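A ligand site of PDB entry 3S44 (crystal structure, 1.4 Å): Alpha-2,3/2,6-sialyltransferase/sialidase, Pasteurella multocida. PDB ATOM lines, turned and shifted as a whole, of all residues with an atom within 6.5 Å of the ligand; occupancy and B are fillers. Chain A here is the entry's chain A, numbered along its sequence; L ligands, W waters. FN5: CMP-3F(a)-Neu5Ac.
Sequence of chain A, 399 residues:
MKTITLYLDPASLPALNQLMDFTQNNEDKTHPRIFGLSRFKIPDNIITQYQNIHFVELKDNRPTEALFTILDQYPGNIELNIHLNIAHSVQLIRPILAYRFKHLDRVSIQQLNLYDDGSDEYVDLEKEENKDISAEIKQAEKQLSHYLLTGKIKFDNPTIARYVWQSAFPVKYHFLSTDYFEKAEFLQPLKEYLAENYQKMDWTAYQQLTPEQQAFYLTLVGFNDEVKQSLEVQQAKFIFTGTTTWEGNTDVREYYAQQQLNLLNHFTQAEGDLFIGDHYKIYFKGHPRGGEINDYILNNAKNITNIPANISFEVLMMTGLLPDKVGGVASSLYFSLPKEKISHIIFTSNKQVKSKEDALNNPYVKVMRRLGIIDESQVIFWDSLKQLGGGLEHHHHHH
A ring nitrogen (NE2) of His 287 is in hydrogen-bond range of an oxygen (O3P) of the ligand (2.7 Å). The backbone carbonyl oxygen (O) of Lys 285 is in hydrogen-bond range of a nitrogen (N4) of the ligand (3.0 Å). The side-chain amino group (NZ) of Lys 285 is in hydrogen-bond range of an oxygen (O2) of the ligand, 2.9 Å away. A nitrogen (N4) of the ligand lies within hydrogen-bond range of the backbone carbonyl oxygen (O) of Gly 242 (2.9 Å). The side-chain hydroxyl (OG) of Ser 331 is in hydrogen-bond range of an oxygen (O1P) of the ligand (3.3 Å).
N of Arg 289 is in hydrogen-bond range of ND1 of His 287 (3.0 Å). O of Lys 285 sits at hydrogen-bond distance from N of Gly 242 (3.0 Å). NZ of Lys 285 is in hydrogen-bond range of O of Ile 311 (2.8 Å). The side-chain amino group (NZ) of Lys 285 sits at hydrogen-bond distance from the backbone carbonyl oxygen (O) of Ala 309 (3.0 Å). The backbone carbonyl oxygen (O) of Phe 240 sits at hydrogen-bond distance from the backbone NH (N) of Lys 285. The side-chain hydroxyl (OG) of Ser 331 sits close to the backbone NH (N) of Leu 333, 3.4 Å away. The backbone NH (N) of Ser 331 sits close to the side-chain hydroxyl (OH) of Tyr 364, 3.2 Å away. O of Val 329 lies within hydrogen-bond range of OG1 of Thr 241 (2.9 Å).
C of Thr 241 touches N4 of the ligand, at 3.8 Å. Gly 286 touches the ligand. Pro 288 touches the ligand (CD to C2, 3.5 Å). Leu 333 touches the ligand. Hydrophobic or aromatic side chains that line the ligand: His 287, Pro 288 and Leu 333.
Water W7 bridges an oxygen (O3P) of the ligand (2.6 Å) and the guanidinium group (NH2) of Arg 289 (3.0 Å). Water W6 lies within hydrogen-bond range of the side-chain carboxylate (OE1) of Glu 314 (2.7 Å) and an oxygen (O2') of the ligand (2.8 Å). Water W1 bridges OG1 of Thr 243 and O1P of the ligand. Water W3 bridges O3' of the ligand (3.0 Å) and OG of Ser 332 (3.3 Å). Water W9 lies within hydrogen-bond range of the backbone carbonyl oxygen (O) of Ala 330 (2.8 Å) and an oxygen (O1P) of the ligand (3.0 Å). Water W5 lies within hydrogen-bond range of the backbone carbonyl oxygen (O) of Ala 309, an oxygen (O2) of the ligand and the side-chain amino group (NZ) of Lys 285.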
ATOM      1  N   SER A  12     -15.496 -26.740 -12.353  1.00  0.00           N
ATOM      2  CA  SER A  12     -16.662 -27.507 -12.829  1.00  0.00           C
ATOM      3  C   SER A  12     -16.588 -27.904 -14.278  1.00  0.00           C
ATOM      4  O   SER A  12     -16.823 -29.048 -14.629  1.00  0.00           O
ATOM      5  CB  SER A  12     -17.959 -26.700 -12.641  1.00  0.00           C
ATOM      6  OG  SER A  12     -18.244 -26.500 -11.269  1.00  0.00           O
ATOM      7  N   PHE A 240     -34.230 -17.468 -14.846  1.00  0.00           N
ATOM      8  CA  PHE A 240     -33.664 -16.325 -14.133  1.00  0.00           C
ATOM      9  C   PHE A 240     -32.493 -16.753 -13.282  1.00  0.00           C
ATOM     10  O   PHE A 240     -32.599 -17.721 -12.537  1.00  0.00           O
ATOM     11  CB  PHE A 240     -34.748 -15.774 -13.197  1.00  0.00           C
ATOM     12  CG  PHE A 240     -34.357 -14.523 -12.440  1.00  0.00           C
ATOM     13  CD1 PHE A 240     -34.531 -13.274 -13.031  1.00  0.00           C
ATOM     14  CD2 PHE A 240     -33.823 -14.588 -11.141  1.00  0.00           C
ATOM     15  CE1 PHE A 240     -34.183 -12.119 -12.348  1.00  0.00           C
ATOM     16  CE2 PHE A 240     -33.490 -13.410 -10.442  1.00  0.00           C
ATOM     17  CZ  PHE A 240     -33.669 -12.184 -11.062  1.00  0.00           C
ATOM     18  N   THR A 241     -31.391 -16.011 -13.407  1.00  0.00           N
ATOM     19  CA  THR A 241     -30.186 -16.259 -12.612  1.00  0.00           C
ATOM     20  C   THR A 241     -30.192 -15.517 -11.274  1.00  0.00           C
ATOM     21  O   THR A 241     -30.052 -14.284 -11.224  1.00  0.00           O
ATOM     22  CB  THR A 241     -28.940 -15.921 -13.413  1.00  0.00           C
ATOM     23  OG1 THR A 241     -29.023 -14.577 -13.927  1.00  0.00           O
ATOM     24  CG2 THR A 241     -28.739 -16.876 -14.560  1.00  0.00           C
ATOM     25  N   GLY A 242     -30.398 -16.267 -10.186  1.00  0.00           N
ATOM     26  CA  GLY A 242     -30.464 -15.659  -8.881  1.00  0.00           C
ATOM     27  C   GLY A 242     -29.080 -15.281  -8.377  1.00  0.00           C
ATOM     28  O   GLY A 242     -28.038 -15.677  -8.914  1.00  0.00           O
ATOM     29  N   THR A 243     -29.088 -14.452  -7.336  1.00  0.00           N
ATOM     30  CA  THR A 243     -27.841 -14.087  -6.677  1.00  0.00           C
ATOM     31  C   THR A 243     -28.017 -14.241  -5.157  1.00  0.00           C
ATOM     32  O   THR A 243     -29.031 -14.744  -4.680  1.00  0.00           O
ATOM     33  CB  THR A 243     -27.405 -12.654  -7.096  1.00  0.00           C
ATOM     34  OG1 THR A 243     -26.059 -12.423  -6.698  1.00  0.00           O
ATOM     35  CG2 THR A 243     -28.340 -11.549  -6.511  1.00  0.00           C
ATOM     36  N   THR A 244     -26.992 -13.821  -4.410  1.00  0.00           N
ATOM     37  CA  THR A 244     -27.072 -13.747  -2.931  1.00  0.00           C
ATOM     38  C   THR A 244     -27.518 -12.348  -2.486  1.00  0.00           C
ATOM     39  O   THR A 244     -28.713 -12.032  -2.575  1.00  0.00           O
ATOM     40  CB  THR A 244     -25.742 -14.202  -2.305  1.00  0.00           C
ATOM     41  OG1 THR A 244     -24.698 -13.400  -2.843  1.00  0.00           O
ATOM     42  CG2 THR A 244     -25.459 -15.663  -2.690  1.00  0.00           C
ATOM     43  N   LYS A 285     -33.115 -20.361 -11.350  1.00  0.00           N
ATOM     44  CA  LYS A 285     -31.879 -21.075 -11.029  1.00  0.00           C
ATOM     45  C   LYS A 285     -31.145 -20.255  -9.968  1.00  0.00           C
ATOM     46  O   LYS A 285     -30.417 -19.307 -10.274  1.00  0.00           O
ATOM     47  CB  LYS A 285     -31.036 -21.274 -12.307  1.00  0.00           C
ATOM     48  CG  LYS A 285     -30.376 -22.657 -12.418  1.00  0.00           C
ATOM     49  CD  LYS A 285     -29.490 -22.996 -11.227  1.00  0.00           C
ATOM     50  CE  LYS A 285     -28.158 -22.278 -11.293  1.00  0.00           C
ATOM     51  NZ  LYS A 285     -27.258 -22.707 -10.168  1.00  0.00           N
ATOM     52  N   GLY A 286     -31.355 -20.631  -8.703  1.00  0.00           N
ATOM     53  CA  GLY A 286     -30.718 -19.891  -7.608  1.00  0.00           C
ATOM     54  C   GLY A 286     -29.215 -20.029  -7.558  1.00  0.00           C
ATOM     55  O   GLY A 286     -28.634 -20.986  -8.114  1.00  0.00           O
ATOM     56  N   HIS A 287     -28.576 -19.017  -6.966  1.00  0.00           N
ATOM     57  CA  HIS A 287     -27.144 -19.078  -6.653  1.00  0.00           C
ATOM     58  C   HIS A 287     -26.867 -20.265  -5.707  1.00  0.00           C
ATOM     59  O   HIS A 287     -27.660 -20.510  -4.783  1.00  0.00           O
ATOM     60  CB  HIS A 287     -26.749 -17.725  -6.054  1.00  0.00           C
ATOM     61  CG  HIS A 287     -25.286 -17.536  -5.908  1.00  0.00           C
ATOM     62  ND1 HIS A 287     -24.511 -18.246  -5.009  1.00  0.00           N
ATOM     63  CD2 HIS A 287     -24.438 -16.685  -6.541  1.00  0.00           C
ATOM     64  CE1 HIS A 287     -23.262 -17.846  -5.100  1.00  0.00           C
ATOM     65  NE2 HIS A 287     -23.188 -16.896  -6.015  1.00  0.00           N
ATOM     66  N   PRO A 288     -25.784 -21.019  -5.961  1.00  0.00           N
ATOM     67  CA  PRO A 288     -25.532 -22.183  -5.114  1.00  0.00           C
ATOM     68  C   PRO A 288     -25.378 -21.833  -3.626  1.00  0.00           C
ATOM     69  O   PRO A 288     -25.567 -22.722  -2.797  1.00  0.00           O
ATOM     70  CB  PRO A 288     -24.228 -22.795  -5.672  1.00  0.00           C
ATOM     71  CG  PRO A 288     -23.664 -21.782  -6.575  1.00  0.00           C
ATOM     72  CD  PRO A 288     -24.800 -20.884  -7.055  1.00  0.00           C
ATOM     73  N   ARG A 289     -25.060 -20.587  -3.294  1.00  0.00           N
ATOM     74  CA  ARG A 289     -24.949 -20.193  -1.899  1.00  0.00           C
ATOM     75  C   ARG A 289     -26.141 -19.352  -1.475  1.00  0.00           C
ATOM     76  O   ARG A 289     -26.118 -18.749  -0.402  1.00  0.00           O
ATOM     77  CB  ARG A 289     -23.658 -19.425  -1.659  1.00  0.00           C
ATOM     78  CG  ARG A 289     -22.383 -20.245  -1.956  1.00  0.00           C
ATOM     79  CD  ARG A 289     -21.120 -19.528  -1.442  1.00  0.00           C
ATOM     80  NE  ARG A 289     -20.886 -18.297  -2.210  1.00  0.00           N
ATOM     81  CZ  ARG A 289     -21.172 -17.068  -1.780  1.00  0.00           C
ATOM     82  NH1 ARG A 289     -21.653 -16.856  -0.554  1.00  0.00           N
ATOM     83  NH2 ARG A 289     -20.922 -16.030  -2.577  1.00  0.00           N
ATOM     84  N   ALA A 309     -30.344 -25.293  -6.985  1.00  0.00           N
ATOM     85  CA  ALA A 309     -29.235 -24.328  -7.070  1.00  0.00           C
ATOM     86  C   ALA A 309     -27.882 -24.994  -7.255  1.00  0.00           C
ATOM     87  O   ALA A 309     -26.954 -24.362  -7.736  1.00  0.00           O
ATOM     88  CB  ALA A 309     -29.241 -23.436  -5.828  1.00  0.00           C
ATOM     89  N   ASN A 310     -27.784 -26.264  -6.903  1.00  0.00           N
ATOM     90  CA  ASN A 310     -26.549 -27.041  -7.099  1.00  0.00           C
ATOM     91  C   ASN A 310     -26.241 -27.411  -8.558  1.00  0.00           C
ATOM     92  O   ASN A 310     -25.137 -27.845  -8.881  1.00  0.00           O
ATOM     93  CB  ASN A 310     -26.449 -28.249  -6.133  1.00  0.00           C
ATOM     94  CG  ASN A 310     -27.731 -29.074  -6.060  1.00  0.00           C
ATOM     95  OD1 ASN A 310     -28.442 -29.238  -7.047  1.00  0.00           O
ATOM     96  ND2 ASN A 310     -27.997 -29.624  -4.870  1.00  0.00           N
ATOM     97  N   ILE A 311     -27.225 -27.219  -9.442  1.00  0.00           N
ATOM     98  CA  ILE A 311     -27.062 -27.561 -10.865  1.00  0.00           C
ATOM     99  C   ILE A 311     -26.504 -26.323 -11.594  1.00  0.00           C
ATOM    100  O   ILE A 311     -27.071 -25.206 -11.497  1.00  0.00           O
ATOM    101  CB  ILE A 311     -28.403 -28.005 -11.481  1.00  0.00           C
ATOM    102  CG1 ILE A 311     -28.758 -29.404 -10.946  1.00  0.00           C
ATOM    103  CG2 ILE A 311     -28.361 -27.974 -13.015  1.00  0.00           C
ATOM    104  CD1 ILE A 311     -30.150 -29.864 -11.291  1.00  0.00           C
ATOM    105  N   SER A 312     -25.415 -26.494 -12.347  1.00  0.00           N
ATOM    106  CA  SER A 312     -24.752 -25.400 -13.057  1.00  0.00           C
ATOM    107  C   SER A 312     -25.330 -25.162 -14.434  1.00  0.00           C
ATOM    108  O   SER A 312     -25.907 -26.066 -15.080  1.00  0.00           O
ATOM    109  CB  SER A 312     -23.249 -25.686 -13.194  1.00  0.00           C
ATOM    110  OG  SER A 312     -22.972 -26.835 -14.015  1.00  0.00           O
ATOM    111  N   PHE A 313     -25.114 -23.955 -14.945  1.00  0.00           N
ATOM    112  CA  PHE A 313     -25.424 -23.721 -16.357  1.00  0.00           C
ATOM    113  C   PHE A 313     -24.546 -24.542 -17.291  1.00  0.00           C
ATOM    114  O   PHE A 313     -24.973 -24.914 -18.395  1.00  0.00           O
ATOM    115  CB  PHE A 313     -25.398 -22.211 -16.665  1.00  0.00           C
ATOM    116  CG  PHE A 313     -26.634 -21.523 -16.215  1.00  0.00           C
ATOM    117  CD1 PHE A 313     -27.712 -21.356 -17.102  1.00  0.00           C
ATOM    118  CD2 PHE A 313     -26.776 -21.104 -14.902  1.00  0.00           C
ATOM    119  CE1 PHE A 313     -28.889 -20.758 -16.682  1.00  0.00           C
ATOM    120  CE2 PHE A 313     -27.979 -20.476 -14.473  1.00  0.00           C
ATOM    121  CZ  PHE A 313     -29.025 -20.318 -15.372  1.00  0.00           C
ATOM    122  N   GLU A 314     -23.343 -24.870 -16.826  1.00  0.00           N
ATOM    123  CA  GLU A 314     -22.453 -25.690 -17.635  1.00  0.00           C
ATOM    124  C   GLU A 314     -23.034 -27.089 -17.841  1.00  0.00           C
ATOM    125  O   GLU A 314     -23.016 -27.618 -18.957  1.00  0.00           O
ATOM    126  CB  GLU A 314     -21.064 -25.707 -17.004  1.00  0.00           C
ATOM    127  CG  GLU A 314     -20.323 -24.369 -17.089  1.00  0.00           C
ATOM    128  CD  GLU A 314     -20.755 -23.313 -16.036  1.00  0.00           C
ATOM    129  OE1 GLU A 314     -21.483 -23.644 -15.091  1.00  0.00           O
ATOM    130  OE2 GLU A 314     -20.332 -22.137 -16.165  1.00  0.00           O
ATOM    131  N   VAL A 329     -29.553 -11.714 -12.629  1.00  0.00           N
ATOM    132  CA  VAL A 329     -28.390 -11.081 -12.026  1.00  0.00           C
ATOM    133  C   VAL A 329     -27.106 -11.625 -12.644  1.00  0.00           C
ATOM    134  O   VAL A 329     -26.981 -12.830 -12.890  1.00  0.00           O
ATOM    135  CB  VAL A 329     -28.374 -11.198 -10.489  1.00  0.00           C
ATOM    136  CG1 VAL A 329     -27.104 -10.562  -9.908  1.00  0.00           C
ATOM    137  CG2 VAL A 329     -29.641 -10.556  -9.883  1.00  0.00           C
ATOM    138  N   ALA A 330     -26.169 -10.699 -12.862  1.00  0.00           N
ATOM    139  CA  ALA A 330     -24.881 -10.990 -13.506  1.00  0.00           C
ATOM    140  C   ALA A 330     -24.081 -12.036 -12.761  1.00  0.00           C
ATOM    141  O   ALA A 330     -24.126 -12.110 -11.548  1.00  0.00           O
ATOM    142  CB  ALA A 330     -24.064  -9.710 -13.586  1.00  0.00           C
ATOM    143  N   SER A 331     -23.407 -12.862 -13.536  1.00  0.00           N
ATOM    144  CA  SER A 331     -22.413 -13.833 -13.038  1.00  0.00           C
ATOM    145  C   SER A 331     -21.527 -14.202 -14.205  1.00  0.00           C
ATOM    146  O   SER A 331     -21.960 -14.103 -15.374  1.00  0.00           O
ATOM    147  CB  SER A 331     -23.160 -15.068 -12.588  1.00  0.00           C
ATOM    148  OG  SER A 331     -22.280 -16.131 -12.243  1.00  0.00           O
ATOM    149  N   SER A 332     -20.318 -14.690 -13.907  1.00  0.00           N
ATOM    150  CA  SER A 332     -19.424 -15.146 -14.987  1.00  0.00           C
ATOM    151  C   SER A 332     -19.998 -16.308 -15.792  1.00  0.00           C
ATOM    152  O   SER A 332     -19.529 -16.568 -16.891  1.00  0.00           O
ATOM    153  CB  SER A 332     -18.050 -15.551 -14.447  1.00  0.00           C
ATOM    154  OG  SER A 332     -18.170 -16.668 -13.602  1.00  0.00           O
ATOM    155  N   LEU A 333     -21.040 -16.964 -15.286  1.00  0.00           N
ATOM    156  CA  LEU A 333     -21.708 -18.034 -16.036  1.00  0.00           C
ATOM    157  C   LEU A 333     -22.192 -17.566 -17.421  1.00  0.00           C
ATOM    158  O   LEU A 333     -22.295 -18.356 -18.364  1.00  0.00           O
ATOM    159  CB  LEU A 333     -22.859 -18.636 -15.205  1.00  0.00           C
ATOM    160  CG  LEU A 333     -24.103 -17.757 -15.066  1.00  0.00           C
ATOM    161  CD1 LEU A 333     -25.083 -17.981 -16.253  1.00  0.00           C
ATOM    162  CD2 LEU A 333     -24.809 -18.057 -13.752  1.00  0.00           C
ATOM    163  N   TYR A 364     -15.179  -9.952 -17.531  1.00  0.00           N
ATOM    164  CA  TYR A 364     -15.786 -10.883 -18.487  1.00  0.00           C
ATOM    165  C   TYR A 364     -16.755 -10.185 -19.447  1.00  0.00           C
ATOM    166  O   TYR A 364     -16.840 -10.564 -20.593  1.00  0.00           O
ATOM    167  CB  TYR A 364     -16.400 -12.132 -17.842  1.00  0.00           C
ATOM    168  CG  TYR A 364     -17.559 -11.902 -16.891  1.00  0.00           C
ATOM    169  CD1 TYR A 364     -18.867 -11.759 -17.400  1.00  0.00           C
ATOM    170  CD2 TYR A 364     -17.370 -11.829 -15.501  1.00  0.00           C
ATOM    171  CE1 TYR A 364     -19.931 -11.540 -16.552  1.00  0.00           C
ATOM    172  CE2 TYR A 364     -18.433 -11.610 -14.653  1.00  0.00           C
ATOM    173  CZ  TYR A 364     -19.715 -11.435 -15.196  1.00  0.00           C
ATOM    174  OH  TYR A 364     -20.766 -11.216 -14.353  1.00  0.00           O
HETATM  175  P   FN5 L   1     -20.942 -15.469  -8.499  1.00  0.00           P
HETATM  176  N1  FN5 L   1     -23.790 -19.478 -10.241  1.00  0.00           N
HETATM  177  C2  FN5 L   1     -24.847 -20.342 -10.529  1.00  0.00           C
HETATM  178  O2  FN5 L   1     -24.691 -21.568 -10.754  1.00  0.00           O
HETATM  179  N3  FN5 L   1     -26.132 -19.885 -10.577  1.00  0.00           N
HETATM  180  C4  FN5 L   1     -26.346 -18.585 -10.320  1.00  0.00           C
HETATM  181  N4  FN5 L   1     -27.619 -18.142 -10.373  1.00  0.00           N
HETATM  182  C5  FN5 L   1     -25.326 -17.698 -10.030  1.00  0.00           C
HETATM  183  C6  FN5 L   1     -24.014 -18.176  -9.970  1.00  0.00           C
HETATM  184  C1' FN5 L   1     -22.438 -20.024 -10.108  1.00  0.00           C
HETATM  185  O2P FN5 L   1     -19.824 -14.553  -8.986  1.00  0.00           O
HETATM  186  C2' FN5 L   1     -21.434 -19.426 -11.072  1.00  0.00           C
HETATM  187  O2' FN5 L   1     -21.369 -20.197 -12.281  1.00  0.00           O
HETATM  188  O1P FN5 L   1     -22.200 -14.975  -9.144  1.00  0.00           O
HETATM  189  C3' FN5 L   1     -20.146 -19.387 -10.283  1.00  0.00           C
HETATM  190  O3' FN5 L   1     -19.470 -20.610 -10.528  1.00  0.00           O
HETATM  191  O3P FN5 L   1     -21.114 -15.483  -6.988  1.00  0.00           O
HETATM  192  C4' FN5 L   1     -20.583 -19.367  -8.827  1.00  0.00           C
HETATM  193  O4' FN5 L   1     -22.015 -19.581  -8.800  1.00  0.00           O
HETATM  194  C5' FN5 L   1     -20.246 -18.043  -8.160  1.00  0.00           C
HETATM  195  O5' FN5 L   1     -20.616 -16.961  -9.018  1.00  0.00           O
HETATM  196  O   HOH W   1     -24.667 -13.858  -8.493  1.00  0.00           O
HETATM  197  O   HOH W   2     -26.273 -14.425 -10.639  1.00  0.00           O
HETATM  198  O   HOH W   3     -17.186 -19.344 -11.903  1.00  0.00           O
HETATM  199  O   HOH W   4     -19.361 -22.869  -9.066  1.00  0.00           O
HETATM  200  O   HOH W   5     -24.391 -24.438  -9.316  1.00  0.00           O
HETATM  201  O   HOH W   6     -20.725 -22.863 -12.598  1.00  0.00           O
HETATM  202  O   HOH W   7     -19.311 -15.771  -5.115  1.00  0.00           O
HETATM  203  O   HOH W   8     -23.689 -21.971 -13.527  1.00  0.00           O
HETATM  204  O   HOH W   9     -21.883 -12.059  -9.919  1.00  0.00           O
HETATM  205  O   HOH W  10     -22.471 -23.593 -10.584  1.00  0.00           O
HETATM  206  O   HOH W  11     -19.587 -20.130 -14.316  1.00  0.00           O
